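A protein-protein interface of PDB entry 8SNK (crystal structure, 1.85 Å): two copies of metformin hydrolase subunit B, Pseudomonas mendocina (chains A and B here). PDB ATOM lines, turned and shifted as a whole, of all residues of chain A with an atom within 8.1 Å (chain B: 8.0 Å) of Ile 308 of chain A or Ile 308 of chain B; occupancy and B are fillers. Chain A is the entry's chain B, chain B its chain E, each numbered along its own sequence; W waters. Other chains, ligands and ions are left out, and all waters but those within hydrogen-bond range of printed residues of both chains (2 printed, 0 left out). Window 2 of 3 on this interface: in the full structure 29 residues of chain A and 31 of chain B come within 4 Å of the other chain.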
ATOM      1  N   SER A 262      -2.883 -19.748   6.118  1.00  0.00           N
ATOM      2  CA  SER A 262      -1.970 -20.779   6.595  1.00  0.00           C
ATOM      3  C   SER A 262      -0.509 -20.380   6.348  1.00  0.00           C
ATOM      4  O   SER A 262       0.354 -20.651   7.202  1.00  0.00           O
ATOM      5  CB  SER A 262      -2.268 -22.146   5.896  1.00  0.00           C
ATOM      6  OG  SER A 262      -3.329 -22.804   6.532  1.00  0.00           O
ATOM      7  N   SER A 263      -0.243 -19.814   5.179  1.00  0.00           N
ATOM      8  CA  SER A 263       1.109 -19.411   4.758  1.00  0.00           C
ATOM      9  C   SER A 263       1.780 -18.531   5.806  1.00  0.00           C
ATOM     10  O   SER A 263       2.975 -18.722   6.078  1.00  0.00           O
ATOM     11  CB  SER A 263       1.101 -18.717   3.427  1.00  0.00           C
ATOM     12  OG  SER A 263       0.358 -17.499   3.518  1.00  0.00           O
ATOM     13  N   THR A 264       1.017 -17.578   6.392  1.00  0.00           N
ATOM     14  CA  THR A 264       1.607 -16.713   7.372  1.00  0.00           C
ATOM     15  C   THR A 264       1.231 -17.072   8.806  1.00  0.00           C
ATOM     16  O   THR A 264       1.754 -16.446   9.716  1.00  0.00           O
ATOM     17  CB  THR A 264       1.389 -15.228   7.090  1.00  0.00           C
ATOM     18  OG1 THR A 264       2.258 -14.550   8.006  1.00  0.00           O
ATOM     19  CG2 THR A 264      -0.014 -14.757   7.322  1.00  0.00           C
ATOM     20  N   ALA A 265       0.457 -18.123   9.022  1.00  0.00           N
ATOM     21  CA  ALA A 265       0.202 -18.659  10.372  1.00  0.00           C
ATOM     22  C   ALA A 265       0.086 -20.175  10.346  1.00  0.00           C
ATOM     23  O   ALA A 265      -1.004 -20.751  10.476  1.00  0.00           O
ATOM     24  CB  ALA A 265      -1.093 -18.018  10.868  1.00  0.00           C
ATOM     25  N   PRO A 266       1.208 -20.908  10.149  1.00  0.00           N
ATOM     26  CA  PRO A 266       1.182 -22.369  10.232  1.00  0.00           C
ATOM     27  C   PRO A 266       1.092 -22.826  11.679  1.00  0.00           C
ATOM     28  O   PRO A 266       0.418 -23.770  11.976  1.00  0.00           O
ATOM     29  CB  PRO A 266       2.510 -22.779   9.527  1.00  0.00           C
ATOM     30  CG  PRO A 266       3.403 -21.577   9.724  1.00  0.00           C
ATOM     31  CD  PRO A 266       2.502 -20.372   9.655  1.00  0.00           C
ATOM     32  N   GLY A 267       1.744 -22.133  12.606  1.00  0.00           N
ATOM     33  CA  GLY A 267       1.843 -22.629  13.962  1.00  0.00           C
ATOM     34  C   GLY A 267       0.712 -22.155  14.868  1.00  0.00           C
ATOM     35  O   GLY A 267       0.922 -21.341  15.771  1.00  0.00           O
ATOM     36  N   VAL A 268      -0.478 -22.631  14.561  1.00  0.00           N
ATOM     37  CA  VAL A 268      -1.680 -22.366  15.317  1.00  0.00           C
ATOM     38  C   VAL A 268      -2.358 -23.706  15.522  1.00  0.00           C
ATOM     39  O   VAL A 268      -2.135 -24.622  14.741  1.00  0.00           O
ATOM     40  CB  VAL A 268      -2.579 -21.326  14.618  1.00  0.00           C
ATOM     41  CG1 VAL A 268      -1.836 -20.025  14.555  1.00  0.00           C
ATOM     42  CG2 VAL A 268      -3.033 -21.749  13.193  1.00  0.00           C
ATOM     43  N   CYS A 303       0.467 -22.267  18.404  1.00  0.00           N
ATOM     44  CA  CYS A 303       0.751 -23.662  18.707  1.00  0.00           C
ATOM     45  C   CYS A 303       2.137 -23.995  18.136  1.00  0.00           C
ATOM     46  O   CYS A 303       2.288 -24.364  16.949  1.00  0.00           O
ATOM     47  CB  CYS A 303      -0.346 -24.530  18.118  1.00  0.00           C
ATOM     48  SG  CYS A 303      -0.211 -26.304  18.514  1.00  0.00           S
ATOM     49  N   PRO A 304       3.193 -23.666  18.882  1.00  0.00           N
ATOM     50  CA  PRO A 304       4.558 -23.677  18.325  1.00  0.00           C
ATOM     51  C   PRO A 304       5.100 -24.977  17.737  1.00  0.00           C
ATOM     52  O   PRO A 304       5.920 -24.923  16.813  1.00  0.00           O
ATOM     53  CB  PRO A 304       5.410 -23.389  19.556  1.00  0.00           C
ATOM     54  CG  PRO A 304       4.529 -22.425  20.329  1.00  0.00           C
ATOM     55  CD  PRO A 304       3.158 -23.020  20.204  1.00  0.00           C
ATOM     56  N   ILE A 305       4.536 -26.107  18.140  1.00  0.00           N
ATOM     57  CA  ILE A 305       4.990 -27.414  17.646  1.00  0.00           C
ATOM     58  C   ILE A 305       4.654 -27.509  16.151  1.00  0.00           C
ATOM     59  O   ILE A 305       5.305 -28.254  15.436  1.00  0.00           O
ATOM     60  CB  ILE A 305       4.405 -28.573  18.498  1.00  0.00           C
ATOM     61  CG1 ILE A 305       4.923 -29.978  18.147  1.00  0.00           C
ATOM     62  CG2 ILE A 305       2.881 -28.583  18.398  1.00  0.00           C
ATOM     63  CD1 ILE A 305       6.316 -30.262  18.537  1.00  0.00           C
ATOM     64  N   PHE A 306       3.687 -26.716  15.640  1.00  0.00           N
ATOM     65  CA  PHE A 306       3.317 -26.731  14.215  1.00  0.00           C
ATOM     66  C   PHE A 306       3.870 -25.558  13.389  1.00  0.00           C
ATOM     67  O   PHE A 306       3.571 -25.422  12.193  1.00  0.00           O
ATOM     68  CB  PHE A 306       1.799 -26.705  14.023  1.00  0.00           C
ATOM     69  CG  PHE A 306       1.032 -27.946  14.448  1.00  0.00           C
ATOM     70  CD1 PHE A 306       1.549 -29.219  14.263  1.00  0.00           C
ATOM     71  CD2 PHE A 306      -0.262 -27.841  14.925  1.00  0.00           C
ATOM     72  CE1 PHE A 306       0.819 -30.357  14.596  1.00  0.00           C
ATOM     73  CE2 PHE A 306      -0.994 -28.974  15.270  1.00  0.00           C
ATOM     74  CZ  PHE A 306      -0.430 -30.235  15.137  1.00  0.00           C
ATOM     75  N   ASP A 307       4.714 -24.726  14.012  1.00  0.00           N
ATOM     76  CA  ASP A 307       5.163 -23.508  13.390  1.00  0.00           C
ATOM     77  C   ASP A 307       6.318 -23.826  12.454  1.00  0.00           C
ATOM     78  O   ASP A 307       6.989 -24.833  12.603  1.00  0.00           O
ATOM     79  CB  ASP A 307       5.535 -22.446  14.434  1.00  0.00           C
ATOM     80  CG  ASP A 307       5.135 -21.032  14.017  1.00  0.00           C
ATOM     81  OD1 ASP A 307       4.669 -20.918  12.878  1.00  0.00           O
ATOM     82  OD2 ASP A 307       5.234 -20.040  14.886  1.00  0.00           O
ATOM     83  N   ILE A 308       6.452 -23.000  11.429  1.00  0.00           N
ATOM     84  CA  ILE A 308       7.510 -23.105  10.423  1.00  0.00           C
ATOM     85  C   ILE A 308       8.459 -21.916  10.664  1.00  0.00           C
ATOM     86  O   ILE A 308       8.044 -20.775  10.436  1.00  0.00           O
ATOM     87  CB  ILE A 308       6.869 -23.112   9.020  1.00  0.00           C
ATOM     88  CG1 ILE A 308       5.937 -24.318   8.801  1.00  0.00           C
ATOM     89  CG2 ILE A 308       7.925 -23.035   7.923  1.00  0.00           C
ATOM     90  CD1 ILE A 308       5.282 -24.353   7.446  1.00  0.00           C
ATOM     91  N   SER A 309       9.625 -22.149  11.312  1.00  0.00           N
ATOM     92  CA  SER A 309      10.591 -21.092  11.615  1.00  0.00           C
ATOM     93  C   SER A 309       9.978 -19.908  12.385  1.00  0.00           C
ATOM     94  O   SER A 309      10.273 -18.738  12.111  1.00  0.00           O
ATOM     95  CB  SER A 309      11.236 -20.637  10.328  1.00  0.00           C
ATOM     96  OG  SER A 309      12.096 -21.632   9.798  1.00  0.00           O
ATOM     97  N   GLY A 310       9.063 -20.200  13.302  1.00  0.00           N
ATOM     98  CA  GLY A 310       8.412 -19.182  14.120  1.00  0.00           C
ATOM     99  C   GLY A 310       7.482 -18.230  13.379  1.00  0.00           C
ATOM    100  O   GLY A 310       7.133 -17.162  13.921  1.00  0.00           O
ATOM    101  N   THR A 311       6.999 -18.619  12.198  1.00  0.00           N
ATOM    102  CA  THR A 311       6.321 -17.679  11.335  1.00  0.00           C
ATOM    103  C   THR A 311       5.073 -17.119  12.015  1.00  0.00           C
ATOM    104  O   THR A 311       4.847 -15.902  12.027  1.00  0.00           O
ATOM    105  CB  THR A 311       5.972 -18.303   9.972  1.00  0.00           C
ATOM    106  OG1 THR A 311       7.175 -18.536   9.226  1.00  0.00           O
ATOM    107  CG2 THR A 311       5.072 -17.401   9.172  1.00  0.00           C
ATOM    108  N   ALA A 312       4.241 -17.995  12.558  1.00  0.00           N
ATOM    109  CA  ALA A 312       2.990 -17.573  13.171  1.00  0.00           C
ATOM    110  C   ALA A 312       3.233 -16.695  14.397  1.00  0.00           C
ATOM    111  O   ALA A 312       2.549 -15.694  14.616  1.00  0.00           O
ATOM    112  CB  ALA A 312       2.128 -18.770  13.452  1.00  0.00           C
ATOM    113  N   ALA A 313       4.144 -17.121  15.257  1.00  0.00           N
ATOM    114  CA  ALA A 313       4.505 -16.430  16.478  1.00  0.00           C
ATOM    115  C   ALA A 313       5.058 -15.045  16.173  1.00  0.00           C
ATOM    116  O   ALA A 313       4.740 -14.089  16.880  1.00  0.00           O
ATOM    117  CB  ALA A 313       5.482 -17.287  17.278  1.00  0.00           C
ATOM    118  N   ARG A 314       5.831 -14.920  15.107  1.00  0.00           N
ATOM    119  CA  ARG A 314       6.444 -13.654  14.732  1.00  0.00           C
ATOM    120  C   ARG A 314       5.384 -12.765  14.103  1.00  0.00           C
ATOM    121  O   ARG A 314       5.376 -11.548  14.332  1.00  0.00           O
ATOM    122  CB  ARG A 314       7.633 -13.828  13.774  1.00  0.00           C
ATOM    123  CG  ARG A 314       8.758 -14.705  14.305  1.00  0.00           C
ATOM    124  CD  ARG A 314       9.787 -15.233  13.281  1.00  0.00           C
ATOM    125  NE  ARG A 314      10.976 -15.832  13.924  1.00  0.00           N
ATOM    126  CZ  ARG A 314      11.836 -15.145  14.689  1.00  0.00           C
ATOM    127  NH1 ARG A 314      11.881 -13.824  14.628  1.00  0.00           N
ATOM    128  NH2 ARG A 314      12.678 -15.764  15.490  1.00  0.00           N
ATOM    129  N   SER B 262       7.724 -12.825   5.347  1.00  0.00           N
ATOM    130  CA  SER B 262       8.218 -13.987   6.097  1.00  0.00           C
ATOM    131  C   SER B 262       7.819 -15.337   5.503  1.00  0.00           C
ATOM    132  O   SER B 262       8.653 -16.236   5.390  1.00  0.00           O
ATOM    133  CB  SER B 262       7.717 -13.912   7.505  1.00  0.00           C
ATOM    134  OG  SER B 262       8.481 -12.969   8.218  1.00  0.00           O
ATOM    135  N   SER B 263       6.542 -15.490   5.123  1.00  0.00           N
ATOM    136  CA  SER B 263       6.028 -16.752   4.585  1.00  0.00           C
ATOM    137  C   SER B 263       6.771 -17.218   3.332  1.00  0.00           C
ATOM    138  O   SER B 263       6.768 -18.411   3.001  1.00  0.00           O
ATOM    139  CB  SER B 263       4.545 -16.647   4.310  1.00  0.00           C
ATOM    140  OG  SER B 263       4.191 -15.402   3.667  1.00  0.00           O
ATOM    141  N   THR B 264       7.359 -16.251   2.618  1.00  0.00           N
ATOM    142  CA  THR B 264       7.970 -16.424   1.310  1.00  0.00           C
ATOM    143  C   THR B 264       9.487 -16.656   1.413  1.00  0.00           C
ATOM    144  O   THR B 264      10.107 -17.074   0.441  1.00  0.00           O
ATOM    145  CB  THR B 264       7.720 -15.111   0.543  1.00  0.00           C
ATOM    146  OG1 THR B 264       6.330 -14.776   0.603  1.00  0.00           O
ATOM    147  CG2 THR B 264       8.121 -15.146  -0.894  1.00  0.00           C
ATOM    148  N   ALA B 265      10.084 -16.246   2.541  1.00  0.00           N
ATOM    149  CA  ALA B 265      11.536 -16.354   2.684  1.00  0.00           C
ATOM    150  C   ALA B 265      11.903 -16.511   4.159  1.00  0.00           C
ATOM    151  O   ALA B 265      12.383 -15.577   4.803  1.00  0.00           O
ATOM    152  CB  ALA B 265      12.201 -15.153   2.030  1.00  0.00           C
ATOM    153  N   PRO B 266      11.567 -17.677   4.749  1.00  0.00           N
ATOM    154  CA  PRO B 266      11.910 -17.981   6.124  1.00  0.00           C
ATOM    155  C   PRO B 266      13.426 -18.081   6.340  1.00  0.00           C
ATOM    156  O   PRO B 266      13.919 -17.581   7.340  1.00  0.00           O
ATOM    157  CB  PRO B 266      11.236 -19.342   6.399  1.00  0.00           C
ATOM    158  CG  PRO B 266      11.026 -19.980   5.038  1.00  0.00           C
ATOM    159  CD  PRO B 266      10.918 -18.815   4.072  1.00  0.00           C
ATOM    160  N   GLY B 267      14.159 -18.727   5.418  1.00  0.00           N
ATOM    161  CA  GLY B 267      15.598 -18.937   5.614  1.00  0.00           C
ATOM    162  C   GLY B 267      16.468 -17.710   5.285  1.00  0.00           C
ATOM    163  O   GLY B 267      17.164 -17.711   4.260  1.00  0.00           O
ATOM    164  N   THR B 271      13.952 -12.423   9.418  1.00  0.00           N
ATOM    165  CA  THR B 271      12.712 -12.350   8.646  1.00  0.00           C
ATOM    166  C   THR B 271      11.812 -11.295   9.253  1.00  0.00           C
ATOM    167  O   THR B 271      11.903 -11.030  10.418  1.00  0.00           O
ATOM    168  CB  THR B 271      11.853 -13.622   8.589  1.00  0.00           C
ATOM    169  OG1 THR B 271      11.479 -14.017   9.909  1.00  0.00           O
ATOM    170  CG2 THR B 271      12.522 -14.784   7.903  1.00  0.00           C
ATOM    171  N   CYS B 303      20.055 -17.688   5.052  1.00  0.00           N
ATOM    172  CA  CYS B 303      20.364 -18.312   6.332  1.00  0.00           C
ATOM    173  C   CYS B 303      19.701 -19.679   6.367  1.00  0.00           C
ATOM    174  O   CYS B 303      18.605 -19.865   6.920  1.00  0.00           O
ATOM    175  CB  CYS B 303      19.944 -17.413   7.476  1.00  0.00           C
ATOM    176  SG  CYS B 303      20.506 -17.931   9.127  1.00  0.00           S
ATOM    177  N   PRO B 304      20.326 -20.639   5.660  1.00  0.00           N
ATOM    178  CA  PRO B 304      19.689 -21.892   5.280  1.00  0.00           C
ATOM    179  C   PRO B 304      19.338 -22.820   6.442  1.00  0.00           C
ATOM    180  O   PRO B 304      18.497 -23.704   6.273  1.00  0.00           O
ATOM    181  CB  PRO B 304      20.699 -22.635   4.390  1.00  0.00           C
ATOM    182  CG  PRO B 304      21.908 -21.734   4.271  1.00  0.00           C
ATOM    183  CD  PRO B 304      21.688 -20.516   5.124  1.00  0.00           C
ATOM    184  N   ILE B 305      19.900 -22.549   7.627  1.00  0.00           N
ATOM    185  CA  ILE B 305      19.589 -23.378   8.786  1.00  0.00           C
ATOM    186  C   ILE B 305      18.179 -23.042   9.283  1.00  0.00           C
ATOM    187  O   ILE B 305      17.590 -23.798  10.043  1.00  0.00           O
ATOM    188  CB  ILE B 305      20.678 -23.234   9.870  1.00  0.00           C
ATOM    189  CG1 ILE B 305      20.506 -24.250  11.010  1.00  0.00           C
ATOM    190  CG2 ILE B 305      20.754 -21.811  10.391  1.00  0.00           C
ATOM    191  CD1 ILE B 305      20.389 -25.702  10.556  1.00  0.00           C
ATOM    192  N   PHE B 306      17.612 -21.926   8.807  1.00  0.00           N
ATOM    193  CA  PHE B 306      16.303 -21.477   9.248  1.00  0.00           C
ATOM    194  C   PHE B 306      15.247 -21.696   8.166  1.00  0.00           C
ATOM    195  O   PHE B 306      14.169 -21.105   8.249  1.00  0.00           O
ATOM    196  CB  PHE B 306      16.377 -20.002   9.653  1.00  0.00           C
ATOM    197  CG  PHE B 306      16.953 -19.739  11.022  1.00  0.00           C
ATOM    198  CD1 PHE B 306      16.484 -20.424  12.138  1.00  0.00           C
ATOM    199  CD2 PHE B 306      17.923 -18.764  11.206  1.00  0.00           C
ATOM    200  CE1 PHE B 306      16.996 -20.159  13.400  1.00  0.00           C
ATOM    201  CE2 PHE B 306      18.440 -18.506  12.467  1.00  0.00           C
ATOM    202  CZ  PHE B 306      17.970 -19.200  13.562  1.00  0.00           C
ATOM    203  N   ASP B 307      15.545 -22.557   7.181  1.00  0.00           N
ATOM    204  CA  ASP B 307      14.797 -22.596   5.932  1.00  0.00           C
ATOM    205  C   ASP B 307      14.011 -23.899   5.913  1.00  0.00           C
ATOM    206  O   ASP B 307      14.448 -24.925   6.440  1.00  0.00           O
ATOM    207  CB  ASP B 307      15.681 -22.526   4.667  1.00  0.00           C
ATOM    208  CG  ASP B 307      15.152 -21.680   3.500  1.00  0.00           C
ATOM    209  OD1 ASP B 307      14.070 -21.057   3.671  1.00  0.00           O
ATOM    210  OD2 ASP B 307      15.885 -21.564   2.430  1.00  0.00           O
ATOM    211  N   ILE B 308      12.861 -23.840   5.236  1.00  0.00           N
ATOM    212  CA  ILE B 308      11.960 -24.978   5.177  1.00  0.00           C
ATOM    213  C   ILE B 308      11.738 -25.348   3.715  1.00  0.00           C
ATOM    214  O   ILE B 308      11.304 -24.514   2.926  1.00  0.00           O
ATOM    215  CB  ILE B 308      10.673 -24.608   5.937  1.00  0.00           C
ATOM    216  CG1 ILE B 308      11.015 -23.900   7.256  1.00  0.00           C
ATOM    217  CG2 ILE B 308       9.813 -25.851   6.153  1.00  0.00           C
ATOM    218  CD1 ILE B 308      11.772 -24.773   8.283  1.00  0.00           C
ATOM    219  N   SER B 309      12.154 -26.552   3.315  1.00  0.00           N
ATOM    220  CA  SER B 309      11.985 -26.961   1.930  1.00  0.00           C
ATOM    221  C   SER B 309      12.800 -26.033   1.035  1.00  0.00           C
ATOM    222  O   SER B 309      12.486 -25.875  -0.144  1.00  0.00           O
ATOM    223  CB  SER B 309      10.539 -26.958   1.493  1.00  0.00           C
ATOM    224  OG  SER B 309       9.703 -27.500   2.498  1.00  0.00           O
ATOM    225  N   GLY B 310      13.832 -25.441   1.648  1.00  0.00           N
ATOM    226  CA  GLY B 310      14.702 -24.466   1.020  1.00  0.00           C
ATOM    227  C   GLY B 310      13.936 -23.289   0.428  1.00  0.00           C
ATOM    228  O   GLY B 310      14.351 -22.763  -0.580  1.00  0.00           O
ATOM    229  N   THR B 311      12.875 -22.822   1.102  1.00  0.00           N
ATOM    230  CA  THR B 311      11.997 -21.816   0.505  1.00  0.00           C
ATOM    231  C   THR B 311      12.742 -20.528   0.149  1.00  0.00           C
ATOM    232  O   THR B 311      12.589 -20.058  -0.968  1.00  0.00           O
ATOM    233  CB  THR B 311      10.787 -21.598   1.409  1.00  0.00           C
ATOM    234  OG1 THR B 311      10.151 -22.882   1.467  1.00  0.00           O
ATOM    235  CG2 THR B 311       9.830 -20.558   0.879  1.00  0.00           C
ATOM    236  N   ALA B 312      13.480 -19.940   1.084  1.00  0.00           N
ATOM    237  CA  ALA B 312      14.203 -18.704   0.806  1.00  0.00           C
ATOM    238  C   ALA B 312      15.244 -18.915  -0.292  1.00  0.00           C
ATOM    239  O   ALA B 312      15.361 -18.089  -1.189  1.00  0.00           O
ATOM    240  CB  ALA B 312      14.801 -18.091   2.062  1.00  0.00           C
ATOM    241  N   ALA B 313      15.951 -20.055  -0.288  1.00  0.00           N
ATOM    242  CA  ALA B 313      17.032 -20.280  -1.234  1.00  0.00           C
ATOM    243  C   ALA B 313      16.475 -20.430  -2.644  1.00  0.00           C
ATOM    244  O   ALA B 313      17.060 -19.943  -3.622  1.00  0.00           O
ATOM    245  CB  ALA B 313      17.864 -21.494  -0.813  1.00  0.00           C
ATOM    246  N   ARG B 314      15.345 -21.130  -2.758  1.00  0.00           N
ATOM    247  CA  ARG B 314      14.644 -21.269  -4.009  1.00  0.00           C
ATOM    248  C   ARG B 314      14.131 -19.923  -4.526  1.00  0.00           C
ATOM    249  O   ARG B 314      14.157 -19.740  -5.733  1.00  0.00           O
ATOM    250  CB  ARG B 314      13.459 -22.220  -3.835  1.00  0.00           C
ATOM    251  CG  ARG B 314      13.886 -23.681  -3.760  1.00  0.00           C
ATOM    252  CD  ARG B 314      12.698 -24.567  -3.493  1.00  0.00           C
ATOM    253  NE  ARG B 314      13.048 -25.640  -2.586  1.00  0.00           N
ATOM    254  CZ  ARG B 314      13.747 -26.712  -2.921  1.00  0.00           C
ATOM    255  NH1 ARG B 314      14.010 -26.959  -4.190  1.00  0.00           N
ATOM    256  NH2 ARG B 314      14.142 -27.555  -1.979  1.00  0.00           N
HETATM  257  O   HOH W   1       6.080 -14.064  10.330  1.00  0.00           O
HETATM  258  O   HOH W   2       0.928 -14.929   2.975  1.00  0.00           O
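O of Phe 306 of chain B sits at hydrogen-bond distance from OG of Ser 309 of chain A (2.6 Å).
Among the printed residues, pairs that only touch across the chains: Ser 263 of chain A with Ser 263 of chain B, Ile 308 of chain A with Ile 308 of chain B, Ser 309 of chain A with Ile 308 of chain B and Arg 314 of chain A with Thr 271 of chain B.
Water W2 lies within hydrogen-bond range of OG of Ser 263 of chain A and OG of Ser 263 of chain B. Water W1 lies within hydrogen-bond range of O of Thr 311 of chain A (2.8 Å) and OG of Ser 262 of chain B (3.4 Å).
Ser 263 of chain B touches its own counterpart, Ser 263 of chain A. Ile 308 of chain A touches its own counterpart, Ile 308 of chain B. Ser 309 of chain A touches Phe 306 of chain B, but with the chains exchanged Phe 306 of chain A does not touch Ser 309 of chain B (11.7 Å). Ser 309 of chain A touches Ile 308 of chain B, but with the chains exchanged Ile 308 of chain A does not touch Ser 309 of chain B (7.2 Å). 18 positions are printed for both chains. Of the 5 pairs that touch across the chains among the printed residues, 2 have their exchanged pair printed and touching as well.
Of chain B, only Ile 308 (3.3 Å) comes within 4 Å of Ile 308 of chain A. Ser 309 of chain A touches just these residues of chain B: Phe 306 (2.6 Å) and Ile 308 (3.5 Å). Of the printed residues of chain A, Thr 271 of chain B touches Arg 314. Of the printed residues of chain A, Phe 306 of chain B touches Ser 309 (2.6 Å). Printed residues of chain A within 4 Å of Ile 308 of chain B: Ile 308 and Ser 309. No residue of chain A comes within 4 Å of Ser 309 of chain B. The nearest residue of chain B that does not touch Ile 308 of chain A is Pro 266 of chain B (5.2 Å).
Printed residues of chain B that touch a printed residue of chain A: Ser 263, Thr 271, Phe 306 and Ile 308. Among the printed residues, no Asp or Glu carboxylate lies within 4 Å of a Lys or Arg side-chain nitrogen of the other chain.
The backbone carbonyl oxygen (O) of Ile 308 of chain A sits at hydrogen-bond distance from the side-chain hydroxyl (OG1) of Thr 311 of chain A, at 2.7 Å. The guanidinium group of Arg 314 of chain A sits at hydrogen-bond distance from the backbone carbonyl oxygen of Ser 309 of chain A (3.5 Å). O of Ile 308 of chain B lies within hydrogen-bond range of OG1 of Thr 311 of chain B, at 2.5 Å.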
